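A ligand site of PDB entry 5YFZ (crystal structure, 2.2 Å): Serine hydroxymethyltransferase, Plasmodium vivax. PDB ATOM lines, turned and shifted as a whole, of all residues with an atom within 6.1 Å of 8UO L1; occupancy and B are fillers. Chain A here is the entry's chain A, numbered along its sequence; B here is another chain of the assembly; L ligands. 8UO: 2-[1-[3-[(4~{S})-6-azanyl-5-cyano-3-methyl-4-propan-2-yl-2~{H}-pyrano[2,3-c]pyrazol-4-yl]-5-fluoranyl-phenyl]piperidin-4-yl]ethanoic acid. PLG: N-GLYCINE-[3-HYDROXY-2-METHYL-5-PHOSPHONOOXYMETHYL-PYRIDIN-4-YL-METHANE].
The backbone carbonyl oxygen of Gly 128 sits at hydrogen-bond distance from a nitrogen (N7) of 8UO L1. An oxygen (O33) of 8UO L1 lies within hydrogen-bond range of the side-chain hydroxyl (OH) of Tyr 63 of chain B (3.4 Å). The side-chain hydroxyl of Tyr 64 of chain B sits at hydrogen-bond distance from an oxygen (O) of PLG L2 (2.8 Å). O1 of 8UO L1 lies within hydrogen-bond range of OG1 of Thr 183, at 3.0 Å. A nitrogen (N11) of 8UO L1 is in hydrogen-bond range of the side-chain carboxylate (OE2) of Glu 56 of chain B. O of Leu 124 lies within hydrogen-bond range of N7 of 8UO L1. The side-chain hydroxyl (OG1) of Thr 357 is in hydrogen-bond range of a nitrogen (N9) of 8UO L1, 3.3 Å away. OXT of PLG L2 is in salt-bridge range of NH1 of Arg 371 (2.9 Å).
O of Glu 56 of chain B lies within hydrogen-bond range of N of Tyr 63 of chain B. The side-chain amide nitrogen of Asn 356 lies within hydrogen-bond range of the side-chain hydroxyl of Ser 184, at 3.1 Å. O of Thr 183 is in hydrogen-bond range of NH1 of Arg 371, 3.0 Å away. The backbone carbonyl oxygen (O) of Cys 125 is in hydrogen-bond range of the side-chain hydroxyl (OG1) of Thr 357 (2.7 Å). O of Asn 354 is in hydrogen-bond range of N of Arg 371 (2.7 Å). The backbone NH (N) of Gly 128 sits at hydrogen-bond distance from the backbone carbonyl oxygen (O) of His 123, at 2.9 Å. The side-chain carboxylate (OE1) of Glu 56 of chain B is in hydrogen-bond range of the side-chain hydroxyl (OH) of Tyr 64 of chain B (3.0 Å). O of Gly 127 is in hydrogen-bond range of N of Ser 184 (3.3 Å).
The side-chain amino group of Lys 355 sits close to a fluorine (F21) of 8UO L1. Gly 127 touches 8UO L1 (C to N7, 3.96 Å). CD2 of His 129 touches N12 of 8UO L1 (3.4 Å). CD1 of Leu 130 touches N11 of 8UO L1, at 3.5 Å. Ser 184 touches 8UO L1 (OG to N7, 3.8 Å). Asn 354 touches 8UO L1 (ND2 to C15, 3.5 Å). Asn 356 touches 8UO L1. Cys 364 touches 8UO L1. Arg 371 touches 8UO L1 (NH1 to C22, 3.4 Å). Tyr 64 of chain B touches 8UO L1. Pro 267 of chain B touches 8UO L1. Hydrophobic or aromatic side chains that line 8UO L1: Leu 124, His 129, Leu 130, Tyr 63 of chain B, Tyr 64 of chain B and Pro 267 of chain B. Of the 25 residues printed, 17 come within 4 Å of 8UO L1.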
ATOM      1  N   HIS A 123       9.419  32.851  20.068  1.00  0.00           N
ATOM      2  CA  HIS A 123       9.874  31.768  20.912  1.00  0.00           C
ATOM      3  C   HIS A 123      10.708  30.786  20.084  1.00  0.00           C
ATOM      4  O   HIS A 123      10.442  30.582  18.891  1.00  0.00           O
ATOM      5  CB  HIS A 123       8.655  31.058  21.528  1.00  0.00           C
ATOM      6  CG  HIS A 123       8.949  30.330  22.795  1.00  0.00           C
ATOM      7  ND1 HIS A 123       9.539  29.100  22.816  1.00  0.00           N
ATOM      8  CD2 HIS A 123       8.718  30.657  24.090  1.00  0.00           C
ATOM      9  CE1 HIS A 123       9.669  28.692  24.064  1.00  0.00           C
ATOM     10  NE2 HIS A 123       9.193  29.622  24.861  1.00  0.00           N
ATOM     11  N   LEU A 124      11.724  30.207  20.722  1.00  0.00           N
ATOM     12  CA  LEU A 124      12.665  29.278  20.076  1.00  0.00           C
ATOM     13  C   LEU A 124      11.903  28.119  19.465  1.00  0.00           C
ATOM     14  O   LEU A 124      12.048  27.826  18.280  1.00  0.00           O
ATOM     15  CB  LEU A 124      13.690  28.753  21.094  1.00  0.00           C
ATOM     16  CG  LEU A 124      14.769  27.767  20.619  1.00  0.00           C
ATOM     17  CD1 LEU A 124      15.972  28.484  20.052  1.00  0.00           C
ATOM     18  CD2 LEU A 124      15.199  26.848  21.756  1.00  0.00           C
ATOM     19  N   CYS A 125      11.091  27.464  20.290  1.00  0.00           N
ATOM     20  CA  CYS A 125      10.142  26.419  19.877  1.00  0.00           C
ATOM     21  C   CYS A 125       9.254  26.721  18.638  1.00  0.00           C
ATOM     22  O   CYS A 125       8.832  25.792  17.957  1.00  0.00           O
ATOM     23  CB  CYS A 125       9.280  26.026  21.083  1.00  0.00           C
ATOM     24  SG  CYS A 125      10.264  25.582  22.552  1.00  0.00           S
ATOM     25  N   SER A 126       8.979  27.990  18.360  1.00  0.00           N
ATOM     26  CA  SER A 126       8.205  28.392  17.180  1.00  0.00           C
ATOM     27  C   SER A 126       9.022  28.853  15.985  1.00  0.00           C
ATOM     28  O   SER A 126       8.452  29.244  14.966  1.00  0.00           O
ATOM     29  CB  SER A 126       7.239  29.501  17.587  1.00  0.00           C
ATOM     30  OG  SER A 126       6.445  29.087  18.678  1.00  0.00           O
ATOM     31  N   GLY A 127      10.347  28.829  16.099  1.00  0.00           N
ATOM     32  CA  GLY A 127      11.231  29.244  15.003  1.00  0.00           C
ATOM     33  C   GLY A 127      12.074  30.479  15.253  1.00  0.00           C
ATOM     34  O   GLY A 127      12.799  30.887  14.362  1.00  0.00           O
ATOM     35  N   GLY A 128      12.006  31.053  16.460  1.00  0.00           N
ATOM     36  CA  GLY A 128      12.893  32.164  16.845  1.00  0.00           C
ATOM     37  C   GLY A 128      14.316  31.705  17.198  1.00  0.00           C
ATOM     38  O   GLY A 128      14.568  30.515  17.377  1.00  0.00           O
ATOM     39  N   HIS A 129      15.256  32.650  17.235  1.00  0.00           N
ATOM     40  CA  HIS A 129      16.619  32.393  17.653  1.00  0.00           C
ATOM     41  C   HIS A 129      16.776  32.603  19.140  1.00  0.00           C
ATOM     42  O   HIS A 129      15.999  33.311  19.763  1.00  0.00           O
ATOM     43  CB  HIS A 129      17.618  33.293  16.925  1.00  0.00           C
ATOM     44  CG  HIS A 129      19.038  32.817  17.024  1.00  0.00           C
ATOM     45  ND1 HIS A 129      20.013  33.526  17.680  1.00  0.00           N
ATOM     46  CD2 HIS A 129      19.628  31.676  16.577  1.00  0.00           C
ATOM     47  CE1 HIS A 129      21.151  32.852  17.638  1.00  0.00           C
ATOM     48  NE2 HIS A 129      20.949  31.744  16.951  1.00  0.00           N
ATOM     49  N   LEU A 130      17.818  31.972  19.684  1.00  0.00           N
ATOM     50  CA  LEU A 130      18.197  32.077  21.098  1.00  0.00           C
ATOM     51  C   LEU A 130      18.372  33.521  21.541  1.00  0.00           C
ATOM     52  O   LEU A 130      17.968  33.873  22.647  1.00  0.00           O
ATOM     53  CB  LEU A 130      19.526  31.382  21.307  1.00  0.00           C
ATOM     54  CG  LEU A 130      19.484  29.868  21.161  1.00  0.00           C
ATOM     55  CD1 LEU A 130      20.887  29.374  20.826  1.00  0.00           C
ATOM     56  CD2 LEU A 130      18.953  29.249  22.446  1.00  0.00           C
ATOM     57  N   PHE A 134      15.258  34.231  24.231  1.00  0.00           N
ATOM     58  CA  PHE A 134      14.855  32.929  24.701  1.00  0.00           C
ATOM     59  C   PHE A 134      15.146  32.710  26.192  1.00  0.00           C
ATOM     60  O   PHE A 134      16.284  32.847  26.629  1.00  0.00           O
ATOM     61  CB  PHE A 134      15.509  31.787  23.920  1.00  0.00           C
ATOM     62  CG  PHE A 134      15.063  30.453  24.413  1.00  0.00           C
ATOM     63  CD1 PHE A 134      13.709  30.102  24.340  1.00  0.00           C
ATOM     64  CD2 PHE A 134      15.941  29.608  25.059  1.00  0.00           C
ATOM     65  CE1 PHE A 134      13.265  28.896  24.859  1.00  0.00           C
ATOM     66  CE2 PHE A 134      15.500  28.403  25.569  1.00  0.00           C
ATOM     67  CZ  PHE A 134      14.167  28.038  25.470  1.00  0.00           C
ATOM     68  N   VAL A 141      18.022  31.116  29.522  1.00  0.00           N
ATOM     69  CA  VAL A 141      18.979  30.444  28.641  1.00  0.00           C
ATOM     70  C   VAL A 141      19.873  31.430  27.847  1.00  0.00           C
ATOM     71  O   VAL A 141      21.071  31.196  27.675  1.00  0.00           O
ATOM     72  CB  VAL A 141      18.240  29.458  27.701  1.00  0.00           C
ATOM     73  CG1 VAL A 141      19.144  28.841  26.630  1.00  0.00           C
ATOM     74  CG2 VAL A 141      17.554  28.357  28.514  1.00  0.00           C
ATOM     75  N   THR A 183      14.866  31.665  12.669  1.00  0.00           N
ATOM     76  CA  THR A 183      15.862  30.630  12.371  1.00  0.00           C
ATOM     77  C   THR A 183      15.274  29.453  11.580  1.00  0.00           C
ATOM     78  O   THR A 183      15.923  28.925  10.697  1.00  0.00           O
ATOM     79  CB  THR A 183      16.688  30.133  13.583  1.00  0.00           C
ATOM     80  OG1 THR A 183      16.451  28.736  13.827  1.00  0.00           O
ATOM     81  CG2 THR A 183      16.432  30.903  14.790  1.00  0.00           C
ATOM     82  N   SER A 184      14.035  29.075  11.868  1.00  0.00           N
ATOM     83  CA  SER A 184      13.385  27.985  11.127  1.00  0.00           C
ATOM     84  C   SER A 184      11.923  28.296  10.849  1.00  0.00           C
ATOM     85  O   SER A 184      11.040  27.602  11.323  1.00  0.00           O
ATOM     86  CB  SER A 184      13.520  26.691  11.899  1.00  0.00           C
ATOM     87  OG  SER A 184      13.057  26.829  13.227  1.00  0.00           O
ATOM     88  N   ASN A 354      18.927  18.721  10.697  1.00  0.00           N
ATOM     89  CA  ASN A 354      18.746  18.884  12.135  1.00  0.00           C
ATOM     90  C   ASN A 354      17.314  18.714  12.574  1.00  0.00           C
ATOM     91  O   ASN A 354      16.367  19.013  11.845  1.00  0.00           O
ATOM     92  CB  ASN A 354      19.340  20.207  12.663  1.00  0.00           C
ATOM     93  CG  ASN A 354      18.541  21.445  12.239  1.00  0.00           C
ATOM     94  OD1 ASN A 354      18.833  22.042  11.212  1.00  0.00           O
ATOM     95  ND2 ASN A 354      17.560  21.823  13.031  1.00  0.00           N
ATOM     96  N   LYS A 355      17.168  18.180  13.790  1.00  0.00           N
ATOM     97  CA  LYS A 355      15.919  18.122  14.494  1.00  0.00           C
ATOM     98  C   LYS A 355      15.402  19.537  14.798  1.00  0.00           C
ATOM     99  O   LYS A 355      16.185  20.475  15.009  1.00  0.00           O
ATOM    100  CB  LYS A 355      16.060  17.292  15.783  1.00  0.00           C
ATOM    101  CG  LYS A 355      16.993  17.840  16.871  1.00  0.00           C
ATOM    102  CD  LYS A 355      16.924  16.952  18.120  1.00  0.00           C
ATOM    103  CE  LYS A 355      17.188  17.690  19.431  1.00  0.00           C
ATOM    104  NZ  LYS A 355      18.598  18.133  19.560  1.00  0.00           N
ATOM    105  N   ASN A 356      14.080  19.679  14.819  1.00  0.00           N
ATOM    106  CA  ASN A 356      13.434  20.994  14.915  1.00  0.00           C
ATOM    107  C   ASN A 356      12.027  20.838  15.465  1.00  0.00           C
ATOM    108  O   ASN A 356      11.287  19.929  15.079  1.00  0.00           O
ATOM    109  CB  ASN A 356      13.372  21.640  13.528  1.00  0.00           C
ATOM    110  CG  ASN A 356      13.171  23.155  13.605  1.00  0.00           C
ATOM    111  OD1 ASN A 356      12.076  23.614  13.891  1.00  0.00           O
ATOM    112  ND2 ASN A 356      14.235  23.912  13.378  1.00  0.00           N
ATOM    113  N   THR A 357      11.645  21.747  16.353  1.00  0.00           N
ATOM    114  CA  THR A 357      10.274  21.788  16.876  1.00  0.00           C
ATOM    115  C   THR A 357       9.252  22.113  15.780  1.00  0.00           C
ATOM    116  O   THR A 357       9.615  22.547  14.676  1.00  0.00           O
ATOM    117  CB  THR A 357      10.159  22.858  17.950  1.00  0.00           C
ATOM    118  OG1 THR A 357      10.785  24.063  17.473  1.00  0.00           O
ATOM    119  CG2 THR A 357      10.841  22.405  19.226  1.00  0.00           C
ATOM    120  N   CYS A 364      10.825  22.166  24.151  1.00  0.00           N
ATOM    121  CA  CYS A 364      11.854  21.861  23.149  1.00  0.00           C
ATOM    122  C   CYS A 364      12.539  20.498  23.390  1.00  0.00           C
ATOM    123  O   CYS A 364      13.528  20.159  22.715  1.00  0.00           O
ATOM    124  CB  CYS A 364      12.903  22.979  23.089  1.00  0.00           C
ATOM    125  SG  CYS A 364      13.367  23.430  21.396  1.00  0.00           S
ATOM    126  N   VAL A 365      11.999  19.717  24.346  1.00  0.00           N
ATOM    127  CA  VAL A 365      12.452  18.347  24.609  1.00  0.00           C
ATOM    128  C   VAL A 365      11.577  17.454  23.733  1.00  0.00           C
ATOM    129  O   VAL A 365      10.343  17.574  23.756  1.00  0.00           O
ATOM    130  CB  VAL A 365      12.270  17.899  26.082  1.00  0.00           C
ATOM    131  CG1 VAL A 365      13.282  16.810  26.406  1.00  0.00           C
ATOM    132  CG2 VAL A 365      12.385  19.049  27.076  1.00  0.00           C
ATOM    133  N   PRO A 367      11.583  17.233  20.046  1.00  0.00           N
ATOM    134  CA  PRO A 367      10.971  17.918  18.891  1.00  0.00           C
ATOM    135  C   PRO A 367      10.463  16.929  17.841  1.00  0.00           C
ATOM    136  O   PRO A 367      11.095  15.867  17.627  1.00  0.00           O
ATOM    137  CB  PRO A 367      12.113  18.762  18.325  1.00  0.00           C
ATOM    138  CG  PRO A 367      13.352  18.079  18.782  1.00  0.00           C
ATOM    139  CD  PRO A 367      13.024  17.507  20.135  1.00  0.00           C
ATOM    140  N   ARG A 371      14.433  20.007  10.230  1.00  0.00           N
ATOM    141  CA  ARG A 371      14.522  21.133   9.324  1.00  0.00           C
ATOM    142  C   ARG A 371      15.539  20.815   8.260  1.00  0.00           C
ATOM    143  O   ARG A 371      16.628  20.322   8.568  1.00  0.00           O
ATOM    144  CB  ARG A 371      14.934  22.385  10.105  1.00  0.00           C
ATOM    145  CG  ARG A 371      15.049  23.649   9.292  1.00  0.00           C
ATOM    146  CD  ARG A 371      15.695  24.767  10.111  1.00  0.00           C
ATOM    147  NE  ARG A 371      17.142  24.565  10.189  1.00  0.00           N
ATOM    148  CZ  ARG A 371      18.019  25.384  10.762  1.00  0.00           C
ATOM    149  NH1 ARG A 371      17.641  26.546  11.312  1.00  0.00           N
ATOM    150  NH2 ARG A 371      19.317  25.037  10.750  1.00  0.00           N
ATOM    151  N   GLU B  56      27.063  23.772  17.080  1.00  0.00           N
ATOM    152  CA  GLU B  56      26.590  24.353  18.337  1.00  0.00           C
ATOM    153  C   GLU B  56      26.608  23.363  19.479  1.00  0.00           C
ATOM    154  O   GLU B  56      26.301  22.192  19.286  1.00  0.00           O
ATOM    155  CB  GLU B  56      25.182  24.895  18.163  1.00  0.00           C
ATOM    156  CG  GLU B  56      25.069  26.120  17.272  1.00  0.00           C
ATOM    157  CD  GLU B  56      23.645  26.590  17.138  1.00  0.00           C
ATOM    158  OE1 GLU B  56      22.884  25.950  16.372  1.00  0.00           O
ATOM    159  OE2 GLU B  56      23.254  27.564  17.812  1.00  0.00           O
ATOM    160  N   TYR B  63      24.130  19.557  18.999  1.00  0.00           N
ATOM    161  CA  TYR B  63      22.742  19.564  18.595  1.00  0.00           C
ATOM    162  C   TYR B  63      22.535  18.801  17.304  1.00  0.00           C
ATOM    163  O   TYR B  63      21.420  18.353  17.036  1.00  0.00           O
ATOM    164  CB  TYR B  63      22.175  21.007  18.533  1.00  0.00           C
ATOM    165  CG  TYR B  63      21.981  21.500  19.940  1.00  0.00           C
ATOM    166  CD1 TYR B  63      23.040  22.075  20.636  1.00  0.00           C
ATOM    167  CD2 TYR B  63      20.785  21.299  20.626  1.00  0.00           C
ATOM    168  CE1 TYR B  63      22.907  22.478  21.948  1.00  0.00           C
ATOM    169  CE2 TYR B  63      20.644  21.699  21.957  1.00  0.00           C
ATOM    170  CZ  TYR B  63      21.717  22.288  22.607  1.00  0.00           C
ATOM    171  OH  TYR B  63      21.624  22.709  23.894  1.00  0.00           O
ATOM    172  N   TYR B  64      23.602  18.617  16.517  1.00  0.00           N
ATOM    173  CA  TYR B  64      23.531  17.787  15.308  1.00  0.00           C
ATOM    174  C   TYR B  64      24.584  16.707  15.280  1.00  0.00           C
ATOM    175  O   TYR B  64      25.551  16.749  16.026  1.00  0.00           O
ATOM    176  CB  TYR B  64      23.697  18.609  14.016  1.00  0.00           C
ATOM    177  CG  TYR B  64      23.332  20.057  14.071  1.00  0.00           C
ATOM    178  CD1 TYR B  64      22.122  20.483  14.631  1.00  0.00           C
ATOM    179  CD2 TYR B  64      24.163  21.022  13.509  1.00  0.00           C
ATOM    180  CE1 TYR B  64      21.775  21.824  14.648  1.00  0.00           C
ATOM    181  CE2 TYR B  64      23.829  22.358  13.531  1.00  0.00           C
ATOM    182  CZ  TYR B  64      22.629  22.767  14.093  1.00  0.00           C
ATOM    183  OH  TYR B  64      22.310  24.110  14.101  1.00  0.00           O
ATOM    184  N   PHE B 266      28.193  29.116  25.599  1.00  0.00           N
ATOM    185  CA  PHE B 266      26.974  28.737  24.870  1.00  0.00           C
ATOM    186  C   PHE B 266      25.994  28.052  25.818  1.00  0.00           C
ATOM    187  O   PHE B 266      26.419  27.205  26.569  1.00  0.00           O
ATOM    188  CB  PHE B 266      27.322  27.826  23.695  1.00  0.00           C
ATOM    189  CG  PHE B 266      26.122  27.276  22.976  1.00  0.00           C
ATOM    190  CD1 PHE B 266      25.532  26.084  23.392  1.00  0.00           C
ATOM    191  CD2 PHE B 266      25.558  27.948  21.894  1.00  0.00           C
ATOM    192  CE1 PHE B 266      24.436  25.582  22.711  1.00  0.00           C
ATOM    193  CE2 PHE B 266      24.450  27.452  21.230  1.00  0.00           C
ATOM    194  CZ  PHE B 266      23.891  26.264  21.628  1.00  0.00           C
ATOM    195  N   PRO B 267      24.700  28.372  25.774  1.00  0.00           N
ATOM    196  CA  PRO B 267      24.079  29.249  24.771  1.00  0.00           C
ATOM    197  C   PRO B 267      23.766  30.677  25.259  1.00  0.00           C
ATOM    198  O   PRO B 267      23.030  31.410  24.561  1.00  0.00           O
ATOM    199  CB  PRO B 267      22.782  28.506  24.456  1.00  0.00           C
ATOM    200  CG  PRO B 267      22.394  27.966  25.766  1.00  0.00           C
ATOM    201  CD  PRO B 267      23.676  27.506  26.409  1.00  0.00           C
HETATM  202  C4  8UO L   1      17.363  25.201  17.139  1.00  0.00           C
HETATM  203  C14 8UO L   1      17.702  24.548  15.752  1.00  0.00           C
HETATM  204  C5  8UO L   1      18.395  26.242  17.412  1.00  0.00           C
HETATM  205  C6  8UO L   1      18.177  27.672  17.189  1.00  0.00           C
HETATM  206  C8  8UO L   1      14.982  25.065  16.936  1.00  0.00           C
HETATM  207  C13 8UO L   1      20.642  25.035  18.303  1.00  0.00           C
HETATM  208  C15 8UO L   1      18.949  23.650  15.728  1.00  0.00           C
HETATM  209  C16 8UO L   1      17.290  24.224  18.321  1.00  0.00           C
HETATM  210  C20 8UO L   1      17.537  24.583  19.678  1.00  0.00           C
HETATM  211  C19 8UO L   1      17.456  23.635  20.740  1.00  0.00           C
HETATM  212  C18 8UO L   1      16.847  21.976  19.097  1.00  0.00           C
HETATM  213  N11 8UO L   1      20.204  27.502  17.916  1.00  0.00           N
HETATM  214  C2  8UO L   1      15.833  27.191  16.752  1.00  0.00           C
HETATM  215  N7  8UO L   1      14.647  27.758  16.555  1.00  0.00           N
HETATM  216  C3  8UO L   1      15.988  25.850  16.949  1.00  0.00           C
HETATM  217  O1  8UO L   1      16.962  28.095  16.733  1.00  0.00           O
HETATM  218  C10 8UO L   1      19.794  26.214  17.895  1.00  0.00           C
HETATM  219  O33 8UO L   1      20.544  24.913  26.294  1.00  0.00           O
HETATM  220  C31 8UO L   1      19.496  24.623  26.911  1.00  0.00           C
HETATM  221  O32 8UO L   1      19.503  24.118  28.064  1.00  0.00           O
HETATM  222  C29 8UO L   1      18.145  24.863  26.257  1.00  0.00           C
HETATM  223  C26 8UO L   1      18.129  24.379  24.807  1.00  0.00           C
HETATM  224  C25 8UO L   1      16.738  23.974  24.384  1.00  0.00           C
HETATM  225  C24 8UO L   1      16.791  23.211  23.072  1.00  0.00           C
HETATM  226  C27 8UO L   1      18.656  25.413  23.832  1.00  0.00           C
HETATM  227  C28 8UO L   1      18.873  24.765  22.460  1.00  0.00           C
HETATM  228  N23 8UO L   1      17.704  23.916  22.110  1.00  0.00           N
HETATM  229  C30 8UO L   1      17.098  22.331  20.400  1.00  0.00           C
HETATM  230  F21 8UO L   1      16.506  20.730  18.783  1.00  0.00           F
HETATM  231  C17 8UO L   1      16.944  22.890  18.070  1.00  0.00           C
HETATM  232  C22 8UO L   1      17.767  25.517  14.544  1.00  0.00           C
HETATM  233  N9  8UO L   1      14.056  24.357  16.922  1.00  0.00           N
HETATM  234  N12 8UO L   1      19.239  28.437  17.495  1.00  0.00           N
HETATM  235  N1  PLG L   2      20.093  34.864  14.070  1.00  0.00           N
HETATM  236  C2  PLG L   2      19.406  33.891  13.448  1.00  0.00           C
HETATM  237  C2A PLG L   2      18.027  34.160  12.894  1.00  0.00           C
HETATM  238  C3  PLG L   2      20.008  32.549  13.319  1.00  0.00           C
HETATM  239  O3  PLG L   2      19.356  31.528  12.705  1.00  0.00           O
HETATM  240  C4  PLG L   2      21.366  32.347  13.861  1.00  0.00           C
HETATM  241  C4A PLG L   2      22.066  31.017  13.775  1.00  0.00           C
HETATM  242  C5  PLG L   2      22.022  33.500  14.514  1.00  0.00           C
HETATM  243  C6  PLG L   2      21.330  34.709  14.600  1.00  0.00           C
HETATM  244  C5A PLG L   2      23.393  33.393  15.150  1.00  0.00           C
HETATM  245  OP4 PLG L   2      24.496  33.129  14.281  1.00  0.00           O
HETATM  246  P   PLG L   2      25.898  32.756  15.039  1.00  0.00           P
HETATM  247  OP1 PLG L   2      25.933  33.379  16.415  1.00  0.00           O
HETATM  248  OP2 PLG L   2      25.770  31.255  15.132  1.00  0.00           O
HETATM  249  OP3 PLG L   2      26.889  33.332  14.072  1.00  0.00           O
HETATM  250  C   PLG L   2      20.945  27.573  12.913  1.00  0.00           C
HETATM  251  O   PLG L   2      21.549  26.510  12.939  1.00  0.00           O
HETATM  252  OXT PLG L   2      20.147  27.786  12.006  1.00  0.00           O
HETATM  253  CA  PLG L   2      21.219  28.632  13.973  1.00  0.00           C
HETATM  254  N   PLG L   2      21.258  29.927  13.306  1.00  0.00           N
